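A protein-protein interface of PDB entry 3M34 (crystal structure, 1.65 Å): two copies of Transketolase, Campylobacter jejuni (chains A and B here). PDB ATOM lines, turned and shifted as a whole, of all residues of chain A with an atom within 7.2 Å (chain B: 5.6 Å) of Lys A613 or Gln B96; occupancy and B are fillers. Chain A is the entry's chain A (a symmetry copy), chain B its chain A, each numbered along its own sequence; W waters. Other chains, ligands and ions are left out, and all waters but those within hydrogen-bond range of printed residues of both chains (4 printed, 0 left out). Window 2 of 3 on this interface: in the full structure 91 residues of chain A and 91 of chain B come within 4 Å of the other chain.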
ATOM      1  N   ILE A 447       4.536  -0.164  -9.380  1.00  0.00           N
ATOM      2  CA  ILE A 447       4.105   0.826  -8.386  1.00  0.00           C
ATOM      3  C   ILE A 447       3.479   0.239  -7.105  1.00  0.00           C
ATOM      4  O   ILE A 447       3.394   0.930  -6.084  1.00  0.00           O
ATOM      5  CB  ILE A 447       3.166   1.882  -9.019  1.00  0.00           C
ATOM      6  CG1 ILE A 447       1.995   1.212  -9.756  1.00  0.00           C
ATOM      7  CG2 ILE A 447       3.964   2.848  -9.904  1.00  0.00           C
ATOM      8  CD1 ILE A 447       0.793   2.161 -10.076  1.00  0.00           C
ATOM      9  N   GLY A 448       3.001  -1.018  -7.139  1.00  0.00           N
ATOM     10  CA  GLY A 448       2.563  -1.737  -5.938  1.00  0.00           C
ATOM     11  C   GLY A 448       3.572  -1.796  -4.802  1.00  0.00           C
ATOM     12  O   GLY A 448       3.230  -2.121  -3.684  1.00  0.00           O
ATOM     13  N   VAL A 449       4.828  -1.523  -5.125  1.00  0.00           N
ATOM     14  CA  VAL A 449       5.871  -1.384  -4.129  1.00  0.00           C
ATOM     15  C   VAL A 449       5.448  -0.358  -3.098  1.00  0.00           C
ATOM     16  O   VAL A 449       5.687  -0.546  -1.908  1.00  0.00           O
ATOM     17  CB  VAL A 449       7.160  -0.991  -4.795  1.00  0.00           C
ATOM     18  CG1 VAL A 449       8.165  -0.300  -3.787  1.00  0.00           C
ATOM     19  CG2 VAL A 449       7.788  -2.262  -5.492  1.00  0.00           C
ATOM     20  N   GLY A 450       4.807   0.730  -3.540  1.00  0.00           N
ATOM     21  CA  GLY A 450       4.277   1.693  -2.564  1.00  0.00           C
ATOM     22  C   GLY A 450       5.273   2.706  -2.025  1.00  0.00           C
ATOM     23  O   GLY A 450       5.821   3.536  -2.757  1.00  0.00           O
ATOM     24  N   GLU A 451       5.491   2.648  -0.729  1.00  0.00           N
ATOM     25  CA  GLU A 451       6.158   3.715  -0.018  1.00  0.00           C
ATOM     26  C   GLU A 451       7.586   4.030  -0.447  1.00  0.00           C
ATOM     27  O   GLU A 451       8.028   5.185  -0.359  1.00  0.00           O
ATOM     28  CB  GLU A 451       6.090   3.479   1.505  1.00  0.00           C
ATOM     29  CG  GLU A 451       4.651   3.622   2.083  1.00  0.00           C
ATOM     30  CD  GLU A 451       3.876   2.329   2.130  1.00  0.00           C
ATOM     31  OE1 GLU A 451       4.205   1.355   1.378  1.00  0.00           O
ATOM     32  OE2 GLU A 451       2.948   2.299   2.992  1.00  0.00           O
ATOM     33  N   GLU A 610       5.107   7.186  -7.524  1.00  0.00           N
ATOM     34  CA  GLU A 610       4.953   8.076  -6.352  1.00  0.00           C
ATOM     35  C   GLU A 610       5.163   7.298  -5.087  1.00  0.00           C
ATOM     36  O   GLU A 610       4.754   6.146  -4.993  1.00  0.00           O
ATOM     37  CB  GLU A 610       3.537   8.666  -6.330  1.00  0.00           C
ATOM     38  CG  GLU A 610       3.209   9.707  -7.382  1.00  0.00           C
ATOM     39  CD  GLU A 610       3.910  11.038  -7.207  1.00  0.00           C
ATOM     40  OE1 GLU A 610       4.451  11.335  -6.123  1.00  0.00           O
ATOM     41  OE2 GLU A 610       3.924  11.797  -8.194  1.00  0.00           O
ATOM     42  N   SER A 611       5.705   7.956  -4.056  1.00  0.00           N
ATOM     43  CA  SER A 611       5.787   7.349  -2.776  1.00  0.00           C
ATOM     44  C   SER A 611       4.446   7.485  -2.038  1.00  0.00           C
ATOM     45  O   SER A 611       3.994   8.582  -1.817  1.00  0.00           O
ATOM     46  CB  SER A 611       6.925   8.009  -1.976  1.00  0.00           C
ATOM     47  OG  SER A 611       6.942   7.618  -0.605  1.00  0.00           O
ATOM     48  N   GLY A 612       3.837   6.356  -1.725  1.00  0.00           N
ATOM     49  CA  GLY A 612       2.656   6.284  -0.877  1.00  0.00           C
ATOM     50  C   GLY A 612       2.236   4.846  -0.628  1.00  0.00           C
ATOM     51  O   GLY A 612       2.803   3.896  -1.168  1.00  0.00           O
ATOM     52  N   LYS A 613       1.202   4.675   0.195  1.00  0.00           N
ATOM     53  CA  LYS A 613       0.610   3.357   0.355  1.00  0.00           C
ATOM     54  C   LYS A 613       0.247   2.757  -0.993  1.00  0.00           C
ATOM     55  O   LYS A 613      -0.326   3.418  -1.892  1.00  0.00           O
ATOM     56  CB  LYS A 613      -0.627   3.444   1.283  1.00  0.00           C
ATOM     57  CG  LYS A 613      -0.274   3.768   2.737  1.00  0.00           C
ATOM     58  CD  LYS A 613      -1.534   3.797   3.628  1.00  0.00           C
ATOM     59  CE  LYS A 613      -1.247   4.418   5.020  1.00  0.00           C
ATOM     60  NZ  LYS A 613      -0.156   3.743   5.734  1.00  0.00           N
ATOM     61  N   ASP A 614       0.523   1.459  -1.168  1.00  0.00           N
ATOM     62  CA  ASP A 614       0.199   0.765  -2.462  1.00  0.00           C
ATOM     63  C   ASP A 614      -1.199   1.022  -2.968  1.00  0.00           C
ATOM     64  O   ASP A 614      -1.362   1.364  -4.134  1.00  0.00           O
ATOM     65  CB  ASP A 614       0.447  -0.766  -2.438  1.00  0.00           C
ATOM     66  CG  ASP A 614      -0.289  -1.502  -1.311  1.00  0.00           C
ATOM     67  OD1 ASP A 614      -1.006  -0.915  -0.459  1.00  0.00           O
ATOM     68  OD2 ASP A 614      -0.114  -2.731  -1.277  1.00  0.00           O
ATOM     69  N   LYS A 615      -2.192   0.934  -2.095  1.00  0.00           N
ATOM     70  CA  LYS A 615      -3.590   1.189  -2.573  1.00  0.00           C
ATOM     71  C   LYS A 615      -3.788   2.636  -3.022  1.00  0.00           C
ATOM     72  O   LYS A 615      -4.459   2.868  -4.039  1.00  0.00           O
ATOM     73  CB  LYS A 615      -4.587   0.811  -1.499  1.00  0.00           C
ATOM     74  CG  LYS A 615      -4.496  -0.704  -1.179  1.00  0.00           C
ATOM     75  CD  LYS A 615      -5.837  -1.374  -0.740  1.00  0.00           C
ATOM     76  CE  LYS A 615      -5.751  -2.937  -0.828  1.00  0.00           C
ATOM     77  NZ  LYS A 615      -7.127  -3.606  -0.944  1.00  0.00           N
ATOM     78  N   ASP A 616      -3.145   3.571  -2.339  1.00  0.00           N
ATOM     79  CA  ASP A 616      -3.190   4.990  -2.720  1.00  0.00           C
ATOM     80  C   ASP A 616      -2.522   5.207  -4.086  1.00  0.00           C
ATOM     81  O   ASP A 616      -3.039   5.964  -4.944  1.00  0.00           O
ATOM     82  CB  ASP A 616      -2.503   5.850  -1.662  1.00  0.00           C
ATOM     83  CG  ASP A 616      -3.296   5.967  -0.385  1.00  0.00           C
ATOM     84  OD1 ASP A 616      -4.463   5.488  -0.388  1.00  0.00           O
ATOM     85  OD2 ASP A 616      -2.759   6.554   0.601  1.00  0.00           O
ATOM     86  N   VAL A 617      -1.347   4.595  -4.288  1.00  0.00           N
ATOM     87  CA  VAL A 617      -0.620   4.773  -5.538  1.00  0.00           C
ATOM     88  C   VAL A 617      -1.355   4.128  -6.734  1.00  0.00           C
ATOM     89  O   VAL A 617      -1.524   4.715  -7.789  1.00  0.00           O
ATOM     90  CB  VAL A 617       0.817   4.232  -5.410  1.00  0.00           C
ATOM     91  CG1 VAL A 617       1.551   4.410  -6.733  1.00  0.00           C
ATOM     92  CG2 VAL A 617       1.545   4.993  -4.285  1.00  0.00           C
ATOM     93  N   PHE A 618      -1.863   2.919  -6.555  1.00  0.00           N
ATOM     94  CA  PHE A 618      -2.609   2.278  -7.642  1.00  0.00           C
ATOM     95  C   PHE A 618      -3.816   3.143  -8.037  1.00  0.00           C
ATOM     96  O   PHE A 618      -4.090   3.319  -9.220  1.00  0.00           O
ATOM     97  CB  PHE A 618      -3.098   0.878  -7.258  1.00  0.00           C
ATOM     98  CG  PHE A 618      -2.104  -0.210  -7.548  1.00  0.00           C
ATOM     99  CD1 PHE A 618      -1.653  -0.433  -8.846  1.00  0.00           C
ATOM    100  CD2 PHE A 618      -1.639  -1.040  -6.531  1.00  0.00           C
ATOM    101  CE1 PHE A 618      -0.754  -1.472  -9.143  1.00  0.00           C
ATOM    102  CE2 PHE A 618      -0.735  -2.111  -6.826  1.00  0.00           C
ATOM    103  CZ  PHE A 618      -0.275  -2.293  -8.086  1.00  0.00           C
ATOM    104  N   GLU A 619      -4.485   3.710  -7.043  1.00  0.00           N
ATOM    105  CA  GLU A 619      -5.700   4.530  -7.319  1.00  0.00           C
ATOM    106  C   GLU A 619      -5.307   5.828  -8.059  1.00  0.00           C
ATOM    107  O   GLU A 619      -5.907   6.205  -9.059  1.00  0.00           O
ATOM    108  CB  GLU A 619      -6.388   4.874  -6.020  1.00  0.00           C
ATOM    109  CG  GLU A 619      -7.613   5.737  -6.207  1.00  0.00           C
ATOM    110  CD  GLU A 619      -8.732   5.015  -6.918  1.00  0.00           C
ATOM    111  OE1 GLU A 619      -8.934   3.801  -6.713  1.00  0.00           O
ATOM    112  OE2 GLU A 619      -9.482   5.668  -7.658  1.00  0.00           O
ATOM    113  N   LYS B  26       4.794   6.088  12.323  1.00  0.00           N
ATOM    114  CA  LYS B  26       3.488   6.690  11.941  1.00  0.00           C
ATOM    115  C   LYS B  26       3.115   6.222  10.550  1.00  0.00           C
ATOM    116  O   LYS B  26       1.947   5.930  10.251  1.00  0.00           O
ATOM    117  CB  LYS B  26       3.532   8.205  11.986  1.00  0.00           C
ATOM    118  CG  LYS B  26       2.189   8.872  11.689  1.00  0.00           C
ATOM    119  CD  LYS B  26       2.170  10.323  12.054  1.00  0.00           C
ATOM    120  CE  LYS B  26       0.756  10.889  11.868  1.00  0.00           C
ATOM    121  NZ  LYS B  26       0.410  11.017  10.423  1.00  0.00           N
ATOM    122  N   ALA B  27       4.128   6.154   9.686  1.00  0.00           N
ATOM    123  CA  ALA B  27       3.945   5.589   8.329  1.00  0.00           C
ATOM    124  C   ALA B  27       3.761   4.080   8.272  1.00  0.00           C
ATOM    125  O   ALA B  27       3.297   3.500   7.257  1.00  0.00           O
ATOM    126  CB  ALA B  27       5.169   5.994   7.402  1.00  0.00           C
ATOM    127  N   ASN B  28       4.179   3.382   9.339  1.00  0.00           N
ATOM    128  CA  ASN B  28       4.217   1.933   9.338  1.00  0.00           C
ATOM    129  C   ASN B  28       5.043   1.430   8.146  1.00  0.00           C
ATOM    130  O   ASN B  28       4.772   0.387   7.567  1.00  0.00           O
ATOM    131  CB  ASN B  28       2.818   1.291   9.340  1.00  0.00           C
ATOM    132  CG  ASN B  28       2.848  -0.129   9.868  1.00  0.00           C
ATOM    133  OD1 ASN B  28       3.773  -0.495  10.627  1.00  0.00           O
ATOM    134  ND2 ASN B  28       1.855  -0.950   9.471  1.00  0.00           N
ATOM    135  N   LYS B  92       5.260  14.344   9.585  1.00  0.00           N
ATOM    136  CA  LYS B  92       4.191  13.454   9.947  1.00  0.00           C
ATOM    137  C   LYS B  92       3.510  12.816   8.738  1.00  0.00           C
ATOM    138  O   LYS B  92       2.760  11.856   8.904  1.00  0.00           O
ATOM    139  CB  LYS B  92       3.127  14.192  10.778  1.00  0.00           C
ATOM    140  CG  LYS B  92       3.656  14.615  12.138  1.00  0.00           C
ATOM    141  CD  LYS B  92       2.535  15.441  12.855  1.00  0.00           C
ATOM    142  CE  LYS B  92       3.071  16.167  14.109  1.00  0.00           C
ATOM    143  NZ  LYS B  92       1.923  16.888  14.821  1.00  0.00           N
ATOM    144  N   ASN B  93       3.820  13.293   7.546  1.00  0.00           N
ATOM    145  CA  ASN B  93       3.313  12.649   6.307  1.00  0.00           C
ATOM    146  C   ASN B  93       4.396  11.898   5.529  1.00  0.00           C
ATOM    147  O   ASN B  93       4.249  11.657   4.345  1.00  0.00           O
ATOM    148  CB  ASN B  93       2.672  13.706   5.457  1.00  0.00           C
ATOM    149  CG  ASN B  93       1.315  14.120   6.074  1.00  0.00           C
ATOM    150  OD1 ASN B  93       1.200  15.144   6.695  1.00  0.00           O
ATOM    151  ND2 ASN B  93       0.310  13.284   5.873  1.00  0.00           N
ATOM    152  N   PHE B  94       5.461  11.517   6.242  1.00  0.00           N
ATOM    153  CA  PHE B  94       6.464  10.605   5.691  1.00  0.00           C
ATOM    154  C   PHE B  94       5.828   9.435   4.941  1.00  0.00           C
ATOM    155  O   PHE B  94       4.954   8.705   5.437  1.00  0.00           O
ATOM    156  CB  PHE B  94       7.371  10.102   6.817  1.00  0.00           C
ATOM    157  CG  PHE B  94       8.513   9.237   6.390  1.00  0.00           C
ATOM    158  CD1 PHE B  94       9.477   9.759   5.573  1.00  0.00           C
ATOM    159  CD2 PHE B  94       8.682   7.955   6.954  1.00  0.00           C
ATOM    160  CE1 PHE B  94      10.624   8.972   5.257  1.00  0.00           C
ATOM    161  CE2 PHE B  94       9.812   7.162   6.650  1.00  0.00           C
ATOM    162  CZ  PHE B  94      10.766   7.666   5.797  1.00  0.00           C
ATOM    163  N   ARG B  95       6.329   9.232   3.719  1.00  0.00           N
ATOM    164  CA  ARG B  95       5.946   8.102   2.908  1.00  0.00           C
ATOM    165  C   ARG B  95       4.491   8.068   2.447  1.00  0.00           C
ATOM    166  O   ARG B  95       4.051   7.051   1.964  1.00  0.00           O
ATOM    167  CB  ARG B  95       6.370   6.758   3.542  1.00  0.00           C
ATOM    168  CG  ARG B  95       7.897   6.470   3.373  1.00  0.00           C
ATOM    169  CD  ARG B  95       8.392   5.257   4.196  1.00  0.00           C
ATOM    170  NE  ARG B  95       9.749   5.018   3.722  1.00  0.00           N
ATOM    171  CZ  ARG B  95      10.079   4.087   2.834  1.00  0.00           C
ATOM    172  NH1 ARG B  95       9.250   3.069   2.530  1.00  0.00           N
ATOM    173  NH2 ARG B  95      11.284   4.149   2.305  1.00  0.00           N
ATOM    174  N   GLN B  96       3.804   9.204   2.551  1.00  0.00           N
ATOM    175  CA  GLN B  96       2.418   9.295   2.113  1.00  0.00           C
ATOM    176  C   GLN B  96       2.263   9.989   0.779  1.00  0.00           C
ATOM    177  O   GLN B  96       3.036  10.873   0.408  1.00  0.00           O
ATOM    178  CB  GLN B  96       1.608  10.037   3.157  1.00  0.00           C
ATOM    179  CG  GLN B  96       1.657   9.350   4.514  1.00  0.00           C
ATOM    180  CD  GLN B  96       1.407   7.840   4.444  1.00  0.00           C
ATOM    181  OE1 GLN B  96       0.327   7.373   4.041  1.00  0.00           O
ATOM    182  NE2 GLN B  96       2.432   7.048   4.832  1.00  0.00           N
ATOM    183  N   LEU B  97       1.225   9.568   0.053  1.00  0.00           N
ATOM    184  CA  LEU B  97       1.008  10.072  -1.279  1.00  0.00           C
ATOM    185  C   LEU B  97       0.948  11.594  -1.287  1.00  0.00           C
ATOM    186  O   LEU B  97       0.201  12.209  -0.512  1.00  0.00           O
ATOM    187  CB  LEU B  97      -0.279   9.501  -1.862  1.00  0.00           C
ATOM    188  CG  LEU B  97      -0.495   9.816  -3.314  1.00  0.00           C
ATOM    189  CD1 LEU B  97       0.499   9.089  -4.261  1.00  0.00           C
ATOM    190  CD2 LEU B  97      -1.956   9.475  -3.770  1.00  0.00           C
ATOM    191  N   HIS B  98       1.795  12.168  -2.121  1.00  0.00           N
ATOM    192  CA  HIS B  98       1.884  13.596  -2.401  1.00  0.00           C
ATOM    193  C   HIS B  98       2.552  14.406  -1.315  1.00  0.00           C
ATOM    194  O   HIS B  98       2.546  15.663  -1.376  1.00  0.00           O
ATOM    195  CB  HIS B  98       0.556  14.199  -2.852  1.00  0.00           C
ATOM    196  CG  HIS B  98      -0.007  13.513  -4.066  1.00  0.00           C
ATOM    197  ND1 HIS B  98      -1.332  13.156  -4.161  1.00  0.00           N
ATOM    198  CD2 HIS B  98       0.590  13.057  -5.196  1.00  0.00           C
ATOM    199  CE1 HIS B  98      -1.531  12.539  -5.309  1.00  0.00           C
ATOM    200  NE2 HIS B  98      -0.388  12.462  -5.959  1.00  0.00           N
ATOM    201  N   SER B  99       3.171  13.715  -0.348  1.00  0.00           N
ATOM    202  CA  SER B  99       3.873  14.470   0.689  1.00  0.00           C
ATOM    203  C   SER B  99       5.200  15.030   0.164  1.00  0.00           C
ATOM    204  O   SER B  99       5.719  14.601  -0.878  1.00  0.00           O
ATOM    205  CB  SER B  99       4.079  13.670   1.938  1.00  0.00           C
ATOM    206  OG  SER B  99       5.262  12.869   1.809  1.00  0.00           O
ATOM    207  N   THR B 101       7.843  14.406   1.839  1.00  0.00           N
ATOM    208  CA  THR B 101       8.766  13.483   2.561  1.00  0.00           C
ATOM    209  C   THR B 101       8.563  12.071   2.025  1.00  0.00           C
ATOM    210  O   THR B 101       8.234  11.149   2.773  1.00  0.00           O
ATOM    211  CB  THR B 101       8.487  13.566   4.084  1.00  0.00           C
ATOM    212  OG1 THR B 101       7.059  13.486   4.275  1.00  0.00           O
ATOM    213  CG2 THR B 101       9.081  14.880   4.691  1.00  0.00           C
HETATM  214  O   HOH W   1       5.682  11.068  -0.429  1.00  0.00           O
HETATM  215  O   HOH W   2      -0.200   7.152   1.232  1.00  0.00           O
HETATM  216  O   HOH W   3       2.385   4.184   4.810  1.00  0.00           O
HETATM  217  O   HOH W   4       3.931  10.924  -3.392  1.00  0.00           O
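The backbone carbonyl oxygen of Ser A611 lies close to the backbone NH of Leu B97 (3.5 Å).
The backbone carbonyl oxygen (O) of Gln B96 sits close to the backbone carbonyl oxygen (O) of Ser A611, 3.3 Å away.
The backbone carbonyl oxygen (O) of Phe B94 sits at hydrogen-bond distance from the side-chain amide nitrogen (NE2) of Gln B96 (3.1 Å).
N of Arg B95 sits at hydrogen-bond distance from O of Thr B101 (2.9 Å).
O of Gln B96 is in hydrogen-bond range of OG of Ser B99, 3.3 Å away.
The side-chain hydroxyl (OG) of Ser A611 lies within hydrogen-bond range of the backbone carbonyl oxygen (O) of Glu A451, at 2.7 Å.
O of Gly A612 is in hydrogen-bond range of N of Glu A451, 3.0 Å away.
Among the printed residues, merely in contact across the chains: Glu A451 with Arg B95, Glu A610 with Leu B97, Ser A611 with Arg B95, Gly A612 with Arg B95, Gly A612 with Leu B97, Lys A613 with Ala B27, Lys A613 with Gln B96 and Asp A616 with Leu B97.
Gly A448 touches none of the printed residues of chain B.
Val A449 touches none of the printed residues of chain B.
Printed residues of chain B within 4 Å of Glu A451: Arg B95 (3.3 Å).
Of the printed residues of chain B, Asp A616 touches Leu B97 (3.9 Å).
Of the printed residues of chain A, Ala B27 touches Lys A613 (3.8 Å).
Printed residues of chain A within 4 Å of Arg B95: Glu A451, Ser A611 and Gly A612.
Of chain A, only Ser A611 and Lys A613 come within 4 Å of Gln B96.
Printed residues of chain A within 4 Å of Leu B97: Glu A610, Ser A611, Gly A612 and Asp A616.
The nearest printed residue of chain A that does not touch Arg B95 is Lys A613 (4.1 Å).
Of the 12 printed residues of chain B, 4 touch a printed residue of chain A.
Of the 15 printed residues of chain A, 6 touch a printed residue of chain B.
Printed residues of chain A that touch a printed residue of chain B: Glu A451, Glu A610, Ser A611, Gly A612, Lys A613 and Asp A616.
Among the printed residues, 10 pairs touch across the chains.
Among the printed residues, no Asp or Glu carboxylate lies within 4 Å of a Lys or Arg side-chain nitrogen of the other chain.
No position is printed for both chains.
Of the 10 pairs that touch across the chains among the printed residues, none has its exchanged pair printed and touching as well.
Water W3 lies within hydrogen-bond range of the side-chain carboxylate (OE2) of Glu A451 (2.7 Å), the backbone carbonyl oxygen (O) of Ala B27 (2.7 Å), the side-chain amino group (NZ) of Lys A613 (2.7 Å) and the side-chain amide nitrogen (NE2) of Gln B96 (2.9 Å).
Water W2 lies within hydrogen-bond range of the side-chain carboxylate of Asp A616 (2.7 Å), the side-chain amide oxygen of Gln B96 (2.9 Å), the backbone NH of Lys A613 (3.0 Å) and the backbone NH of Leu B97 (3.0 Å).
Water W4 lies within hydrogen-bond range of N of His B98 (2.8 Å), OE1 of Glu A610 (2.8 Å) and O of Ser A611 (2.8 Å).
Water W1 lies within hydrogen-bond range of the backbone carbonyl oxygen of Gln B96 (2.8 Å), the side-chain hydroxyl of Ser B99 (2.9 Å) and the backbone carbonyl oxygen of Ser A611 (3.3 Å).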
